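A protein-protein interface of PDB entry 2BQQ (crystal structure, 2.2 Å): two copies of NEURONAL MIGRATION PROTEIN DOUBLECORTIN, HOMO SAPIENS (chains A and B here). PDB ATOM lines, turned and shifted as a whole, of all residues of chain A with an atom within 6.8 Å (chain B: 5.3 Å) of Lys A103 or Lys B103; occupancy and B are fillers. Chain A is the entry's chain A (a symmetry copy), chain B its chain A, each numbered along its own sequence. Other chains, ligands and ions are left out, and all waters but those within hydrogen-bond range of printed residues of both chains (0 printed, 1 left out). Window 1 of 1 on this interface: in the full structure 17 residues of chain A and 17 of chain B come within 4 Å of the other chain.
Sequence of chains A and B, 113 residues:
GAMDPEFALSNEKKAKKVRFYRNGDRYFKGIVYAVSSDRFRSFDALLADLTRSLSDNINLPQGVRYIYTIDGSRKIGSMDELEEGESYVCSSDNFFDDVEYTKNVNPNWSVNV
The backbone NH of Lys B103 is in hydrogen-bond range of the backbone carbonyl oxygen of Lys A103 (2.8 Å).
ND2 of Asn A104 lies within hydrogen-bond range of O of Tyr B101 (3.1 Å).
The backbone NH (N) of Val B105 sits at hydrogen-bond distance from the backbone carbonyl oxygen (O) of Tyr A101 (2.8 Å).
N of Val A105 lies within hydrogen-bond range of O of Tyr B101.
ND2 of Asn B104 is in hydrogen-bond range of O of Tyr A101 (3.1 Å).
OE1 of Glu A100 is in salt-bridge range of NZ of Lys B29.
OH of Tyr A21 is in hydrogen-bond range of O of Thr A102 (3.0 Å).
O of Lys A29 is in hydrogen-bond range of NH1 of Arg A19, 2.9 Å away.
The side-chain amide oxygen (OD1) of Asn A104 sits close to the backbone carbonyl oxygen (O) of Asn A106, 2.9 Å away.
O of Thr B102 is in hydrogen-bond range of OH of Tyr B21, at 3.0 Å.
The side-chain amide oxygen (OD1) of Asn A104 sits at hydrogen-bond distance from the side-chain hydroxyl (OG) of Ser A110, at 3.3 Å.
Among the printed residues, pairs that only touch across the chains: Tyr A21 with Val B105 (3.6 Å), Lys A29 with Thr B102 (3.6 Å), Glu A100 with Asn B104 (3.3 Å), Thr A102 with Lys B29 (3.6 Å), Thr A102 with Lys B103 (3.2 Å), Lys A103 with Thr B102 (3.2 Å), Lys A103 with Val B105 (3.3 Å), Val A105 with Tyr B21 (3.6 Å), Val A105 with Lys B103 (3.3 Å) and Asn A106 with Tyr B101 (3.9 Å).
Lys A103 touches three residues of chain B.
Lys B103 touches three residues of chain A.
Of the printed residues of chain A, Thr B102 touches Lys A29 and Lys A103.
Of the printed residues of chain B, Glu A100 touches Lys B29 (2.8 Å) and Asn B104 (3.3 Å).
Of the printed residues of chain B, Thr A102 touches Lys B29 and Lys B103.
Of the printed residues of chain A, Asn B104 touches Glu A100 and Tyr A101.
Phe A28 touches none of the printed residues of chain B.
The nearest residue of chain A that does not touch Lys B103 is Tyr A101 (4.2 Å).
The nearest printed residue of chain A that does not touch Asn B104 is Thr A102 (4.2 Å).
Of the 13 printed residues of chain A, 9 touch a printed residue of chain B.
Hydrophobic or aromatic side chains of chain A that line the printed part of chain B: Tyr A21 and Val A105.
Of the 7 printed residues of chain B, 7 touch a printed residue of chain A.
Hydrophobic or aromatic side chains of chain B that line the printed part of chain A: Tyr B21, Tyr B101 and Val B105.
Along chain B the printed residues that touch a printed residue of chain A span positions 21 to 105.
Among the printed residues, Asp or Glu carboxylates within 4 Å of a Lys or Arg side-chain nitrogen of the other chain: Glu A100 with Lys B29.
Tyr A21 touches Val B105, and with the chains exchanged Val A105 touches Tyr B21.
Lys A29 touches Thr B102, and with the chains exchanged Thr A102 touches Lys B29.
Tyr A101 touches Val B105, and with the chains exchanged Val A105 touches Tyr B101.
Lys A103 touches its own counterpart, Lys B103.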
ATOM      1  N   ARG A  19      21.173 -18.873  29.592  1.00  0.00           N
ATOM      2  CA  ARG A  19      20.656 -19.540  28.425  1.00  0.00           C
ATOM      3  C   ARG A  19      20.735 -21.039  28.642  1.00  0.00           C
ATOM      4  O   ARG A  19      21.738 -21.545  29.088  1.00  0.00           O
ATOM      5  CB  ARG A  19      21.388 -19.082  27.159  1.00  0.00           C
ATOM      6  CG  ARG A  19      20.986 -19.849  25.864  1.00  0.00           C
ATOM      7  CD  ARG A  19      21.767 -19.289  24.653  1.00  0.00           C
ATOM      8  NE  ARG A  19      21.372 -17.909  24.324  1.00  0.00           N
ATOM      9  CZ  ARG A  19      20.374 -17.509  23.528  1.00  0.00           C
ATOM     10  NH1 ARG A  19      19.561 -18.335  22.868  1.00  0.00           N
ATOM     11  NH2 ARG A  19      20.171 -16.210  23.370  1.00  0.00           N
ATOM     12  N   TYR A  21      20.485 -24.917  26.976  1.00  0.00           N
ATOM     13  CA  TYR A  21      20.501 -25.799  25.818  1.00  0.00           C
ATOM     14  C   TYR A  21      20.042 -27.190  26.214  1.00  0.00           C
ATOM     15  O   TYR A  21      19.858 -27.455  27.398  1.00  0.00           O
ATOM     16  CB  TYR A  21      21.934 -25.909  25.271  1.00  0.00           C
ATOM     17  CG  TYR A  21      22.443 -24.655  24.620  1.00  0.00           C
ATOM     18  CD1 TYR A  21      23.070 -23.658  25.378  1.00  0.00           C
ATOM     19  CD2 TYR A  21      22.287 -24.461  23.258  1.00  0.00           C
ATOM     20  CE1 TYR A  21      23.543 -22.501  24.767  1.00  0.00           C
ATOM     21  CE2 TYR A  21      22.776 -23.304  22.644  1.00  0.00           C
ATOM     22  CZ  TYR A  21      23.389 -22.329  23.400  1.00  0.00           C
ATOM     23  OH  TYR A  21      23.843 -21.195  22.782  1.00  0.00           O
ATOM     24  N   PHE A  28      19.531 -26.734  18.149  1.00  0.00           N
ATOM     25  CA  PHE A  28      18.735 -25.898  19.043  1.00  0.00           C
ATOM     26  C   PHE A  28      19.607 -24.798  19.678  1.00  0.00           C
ATOM     27  O   PHE A  28      20.603 -25.131  20.307  1.00  0.00           O
ATOM     28  CB  PHE A  28      18.068 -26.768  20.113  1.00  0.00           C
ATOM     29  CG  PHE A  28      17.188 -25.982  21.047  1.00  0.00           C
ATOM     30  CD1 PHE A  28      15.965 -25.495  20.606  1.00  0.00           C
ATOM     31  CD2 PHE A  28      17.601 -25.743  22.344  1.00  0.00           C
ATOM     32  CE1 PHE A  28      15.131 -24.760  21.436  1.00  0.00           C
ATOM     33  CE2 PHE A  28      16.779 -25.009  23.191  1.00  0.00           C
ATOM     34  CZ  PHE A  28      15.549 -24.526  22.737  1.00  0.00           C
ATOM     35  N   LYS A  29      19.251 -23.527  19.513  1.00  0.00           N
ATOM     36  CA  LYS A  29      20.064 -22.385  19.934  1.00  0.00           C
ATOM     37  C   LYS A  29      19.891 -21.893  21.379  1.00  0.00           C
ATOM     38  O   LYS A  29      20.442 -20.853  21.726  1.00  0.00           O
ATOM     39  CB  LYS A  29      19.811 -21.224  18.977  1.00  0.00           C
ATOM     40  CG  LYS A  29      20.373 -21.407  17.582  1.00  0.00           C
ATOM     41  CD  LYS A  29      19.816 -20.395  16.583  1.00  0.00           C
ATOM     42  CE  LYS A  29      18.359 -20.672  16.168  1.00  0.00           C
ATOM     43  NZ  LYS A  29      18.243 -20.370  14.715  1.00  0.00           N
ATOM     44  N   GLY A  30      19.162 -22.632  22.212  1.00  0.00           N
ATOM     45  CA  GLY A  30      18.999 -22.298  23.619  1.00  0.00           C
ATOM     46  C   GLY A  30      17.790 -21.404  23.836  1.00  0.00           C
ATOM     47  O   GLY A  30      17.277 -20.742  22.921  1.00  0.00           O
ATOM     48  N   GLU A 100      28.980 -29.384  19.337  1.00  0.00           N
ATOM     49  CA  GLU A 100      29.024 -27.953  19.105  1.00  0.00           C
ATOM     50  C   GLU A 100      27.691 -27.248  19.373  1.00  0.00           C
ATOM     51  O   GLU A 100      26.907 -27.153  18.447  1.00  0.00           O
ATOM     52  CB  GLU A 100      29.468 -27.771  17.661  1.00  0.00           C
ATOM     53  CG  GLU A 100      30.893 -28.307  17.586  1.00  0.00           C
ATOM     54  CD  GLU A 100      31.576 -28.032  16.277  1.00  0.00           C
ATOM     55  OE1 GLU A 100      30.983 -28.337  15.219  1.00  0.00           O
ATOM     56  OE2 GLU A 100      32.707 -27.506  16.336  1.00  0.00           O
ATOM     57  N   TYR A 101      27.421 -26.761  20.580  1.00  0.00           N
ATOM     58  CA  TYR A 101      26.212 -25.993  20.888  1.00  0.00           C
ATOM     59  C   TYR A 101      26.370 -24.673  20.116  1.00  0.00           C
ATOM     60  O   TYR A 101      27.496 -24.216  19.949  1.00  0.00           O
ATOM     61  CB  TYR A 101      26.051 -25.797  22.410  1.00  0.00           C
ATOM     62  CG  TYR A 101      25.877 -27.161  23.052  1.00  0.00           C
ATOM     63  CD1 TYR A 101      24.639 -27.818  23.056  1.00  0.00           C
ATOM     64  CD2 TYR A 101      26.972 -27.840  23.617  1.00  0.00           C
ATOM     65  CE1 TYR A 101      24.506 -29.084  23.633  1.00  0.00           C
ATOM     66  CE2 TYR A 101      26.821 -29.106  24.192  1.00  0.00           C
ATOM     67  CZ  TYR A 101      25.592 -29.722  24.193  1.00  0.00           C
ATOM     68  OH  TYR A 101      25.490 -30.989  24.752  1.00  0.00           O
ATOM     69  N   THR A 102      25.272 -24.076  19.656  1.00  0.00           N
ATOM     70  CA  THR A 102      25.385 -22.891  18.795  1.00  0.00           C
ATOM     71  C   THR A 102      24.513 -21.699  19.173  1.00  0.00           C
ATOM     72  O   THR A 102      23.524 -21.840  19.872  1.00  0.00           O
ATOM     73  CB  THR A 102      25.054 -23.219  17.325  1.00  0.00           C
ATOM     74  OG1 THR A 102      23.769 -23.829  17.320  1.00  0.00           O
ATOM     75  CG2 THR A 102      26.075 -24.167  16.637  1.00  0.00           C
ATOM     76  N   LYS A 103      24.882 -20.512  18.715  1.00  0.00           N
ATOM     77  CA  LYS A 103      24.062 -19.340  18.950  1.00  0.00           C
ATOM     78  C   LYS A 103      24.069 -18.579  17.639  1.00  0.00           C
ATOM     79  O   LYS A 103      24.967 -18.808  16.819  1.00  0.00           O
ATOM     80  CB  LYS A 103      24.633 -18.460  20.054  1.00  0.00           C
ATOM     81  CG  LYS A 103      25.954 -17.773  19.706  1.00  0.00           C
ATOM     82  CD  LYS A 103      26.266 -16.581  20.595  1.00  0.00           C
ATOM     83  CE  LYS A 103      27.766 -16.455  20.898  1.00  0.00           C
ATOM     84  NZ  LYS A 103      28.367 -15.127  21.302  1.00  0.00           N
ATOM     85  N   ASN A 104      23.090 -17.684  17.511  1.00  0.00           N
ATOM     86  CA  ASN A 104      22.900 -16.789  16.372  1.00  0.00           C
ATOM     87  C   ASN A 104      24.030 -15.778  16.297  1.00  0.00           C
ATOM     88  O   ASN A 104      24.514 -15.345  17.346  1.00  0.00           O
ATOM     89  CB  ASN A 104      21.539 -16.069  16.454  1.00  0.00           C
ATOM     90  CG  ASN A 104      21.397 -14.972  15.410  1.00  0.00           C
ATOM     91  OD1 ASN A 104      21.362 -13.780  15.754  1.00  0.00           O
ATOM     92  ND2 ASN A 104      21.353 -15.349  14.131  1.00  0.00           N
ATOM     93  N   VAL A 105      24.451 -15.436  15.076  1.00  0.00           N
ATOM     94  CA  VAL A 105      25.352 -14.297  14.839  1.00  0.00           C
ATOM     95  C   VAL A 105      24.693 -13.180  14.024  1.00  0.00           C
ATOM     96  O   VAL A 105      25.282 -12.107  13.933  1.00  0.00           O
ATOM     97  CB  VAL A 105      26.732 -14.707  14.250  1.00  0.00           C
ATOM     98  CG1 VAL A 105      27.373 -15.715  15.196  1.00  0.00           C
ATOM     99  CG2 VAL A 105      26.632 -15.325  12.865  1.00  0.00           C
ATOM    100  N   ASN A 106      23.513 -13.394  13.438  1.00  0.00           N
ATOM    101  CA  ASN A 106      22.861 -12.396  12.561  1.00  0.00           C
ATOM    102  C   ASN A 106      22.402 -11.174  13.384  1.00  0.00           C
ATOM    103  O   ASN A 106      21.492 -11.324  14.195  1.00  0.00           O
ATOM    104  CB  ASN A 106      21.766 -13.066  11.699  1.00  0.00           C
ATOM    105  CG  ASN A 106      21.166 -12.180  10.592  1.00  0.00           C
ATOM    106  OD1 ASN A 106      21.396 -10.975  10.482  1.00  0.00           O
ATOM    107  ND2 ASN A 106      20.363 -12.815   9.739  1.00  0.00           N
ATOM    108  N   SER A 110      19.487 -10.658  17.178  1.00  0.00           N
ATOM    109  CA  SER A 110      20.046 -10.542  18.537  1.00  0.00           C
ATOM    110  C   SER A 110      20.502  -9.112  18.806  1.00  0.00           C
ATOM    111  O   SER A 110      20.943  -8.410  17.895  1.00  0.00           O
ATOM    112  CB  SER A 110      21.183 -11.531  18.827  1.00  0.00           C
ATOM    113  OG  SER A 110      20.732 -12.883  18.862  1.00  0.00           O
ATOM    114  N   TYR B  21      29.646 -17.935   5.295  1.00  0.00           N
ATOM    115  CA  TYR B  21      28.449 -18.755   5.405  1.00  0.00           C
ATOM    116  C   TYR B  21      27.814 -18.940   4.039  1.00  0.00           C
ATOM    117  O   TYR B  21      28.248 -18.313   3.078  1.00  0.00           O
ATOM    118  CB  TYR B  21      27.425 -18.056   6.315  1.00  0.00           C
ATOM    119  CG  TYR B  21      27.816 -18.012   7.764  1.00  0.00           C
ATOM    120  CD1 TYR B  21      28.605 -16.968   8.263  1.00  0.00           C
ATOM    121  CD2 TYR B  21      27.410 -19.015   8.629  1.00  0.00           C
ATOM    122  CE1 TYR B  21      28.960 -16.932   9.607  1.00  0.00           C
ATOM    123  CE2 TYR B  21      27.756 -18.969   9.982  1.00  0.00           C
ATOM    124  CZ  TYR B  21      28.534 -17.938  10.461  1.00  0.00           C
ATOM    125  OH  TYR B  21      28.879 -17.923  11.786  1.00  0.00           O
ATOM    126  N   LYS B  29      27.852 -23.687  10.073  1.00  0.00           N
ATOM    127  CA  LYS B  29      28.506 -22.716  10.952  1.00  0.00           C
ATOM    128  C   LYS B  29      29.619 -21.853  10.341  1.00  0.00           C
ATOM    129  O   LYS B  29      30.289 -21.134  11.077  1.00  0.00           O
ATOM    130  CB  LYS B  29      29.054 -23.451  12.171  1.00  0.00           C
ATOM    131  CG  LYS B  29      28.006 -23.968  13.136  1.00  0.00           C
ATOM    132  CD  LYS B  29      28.571 -24.969  14.142  1.00  0.00           C
ATOM    133  CE  LYS B  29      28.876 -26.351  13.536  1.00  0.00           C
ATOM    134  NZ  LYS B  29      28.491 -27.376  14.544  1.00  0.00           N
ATOM    135  N   TYR B 101      21.989 -17.129  11.052  1.00  0.00           N
ATOM    136  CA  TYR B 101      23.286 -17.769  10.823  1.00  0.00           C
ATOM    137  C   TYR B 101      23.841 -18.063  12.226  1.00  0.00           C
ATOM    138  O   TYR B 101      23.562 -17.299  13.143  1.00  0.00           O
ATOM    139  CB  TYR B 101      24.209 -16.868   9.975  1.00  0.00           C
ATOM    140  CG  TYR B 101      23.570 -16.675   8.612  1.00  0.00           C
ATOM    141  CD1 TYR B 101      23.679 -17.645   7.607  1.00  0.00           C
ATOM    142  CD2 TYR B 101      22.795 -15.536   8.331  1.00  0.00           C
ATOM    143  CE1 TYR B 101      23.063 -17.458   6.366  1.00  0.00           C
ATOM    144  CE2 TYR B 101      22.188 -15.363   7.084  1.00  0.00           C
ATOM    145  CZ  TYR B 101      22.320 -16.326   6.111  1.00  0.00           C
ATOM    146  OH  TYR B 101      21.681 -16.128   4.894  1.00  0.00           O
ATOM    147  N   THR B 102      24.605 -19.142  12.389  1.00  0.00           N
ATOM    148  CA  THR B 102      25.039 -19.538  13.736  1.00  0.00           C
ATOM    149  C   THR B 102      26.522 -19.848  13.900  1.00  0.00           C
ATOM    150  O   THR B 102      27.215 -20.136  12.938  1.00  0.00           O
ATOM    151  CB  THR B 102      24.279 -20.782  14.239  1.00  0.00           C
ATOM    152  OG1 THR B 102      24.441 -21.790  13.248  1.00  0.00           O
ATOM    153  CG2 THR B 102      22.763 -20.546  14.488  1.00  0.00           C
ATOM    154  N   LYS B 103      27.020 -19.788  15.126  1.00  0.00           N
ATOM    155  CA  LYS B 103      28.398 -20.156  15.385  1.00  0.00           C
ATOM    156  C   LYS B 103      28.360 -20.960  16.670  1.00  0.00           C
ATOM    157  O   LYS B 103      27.380 -20.850  17.417  1.00  0.00           O
ATOM    158  CB  LYS B 103      29.286 -18.933  15.575  1.00  0.00           C
ATOM    159  CG  LYS B 103      29.001 -18.126  16.843  1.00  0.00           C
ATOM    160  CD  LYS B 103      30.149 -17.215  17.247  1.00  0.00           C
ATOM    161  CE  LYS B 103      29.658 -15.886  17.839  1.00  0.00           C
ATOM    162  NZ  LYS B 103      30.545 -15.071  18.754  1.00  0.00           N
ATOM    163  N   ASN B 104      29.441 -21.708  16.888  1.00  0.00           N
ATOM    164  CA  ASN B 104      29.678 -22.537  18.068  1.00  0.00           C
ATOM    165  C   ASN B 104      29.853 -21.667  19.301  1.00  0.00           C
ATOM    166  O   ASN B 104      30.425 -20.579  19.187  1.00  0.00           O
ATOM    167  CB  ASN B 104      30.909 -23.443  17.871  1.00  0.00           C
ATOM    168  CG  ASN B 104      31.317 -24.158  19.150  1.00  0.00           C
ATOM    169  OD1 ASN B 104      32.381 -23.866  19.720  1.00  0.00           O
ATOM    170  ND2 ASN B 104      30.469 -25.066  19.640  1.00  0.00           N
ATOM    171  N   VAL B 105      29.344 -22.135  20.444  1.00  0.00           N
ATOM    172  CA  VAL B 105      29.651 -21.534  21.752  1.00  0.00           C
ATOM    173  C   VAL B 105      30.428 -22.480  22.671  1.00  0.00           C
ATOM    174  O   VAL B 105      30.902 -22.021  23.706  1.00  0.00           O
ATOM    175  CB  VAL B 105      28.409 -20.925  22.463  1.00  0.00           C
ATOM    176  CG1 VAL B 105      27.782 -19.897  21.530  1.00  0.00           C
ATOM    177  CG2 VAL B 105      27.361 -21.962  22.830  1.00  0.00           C
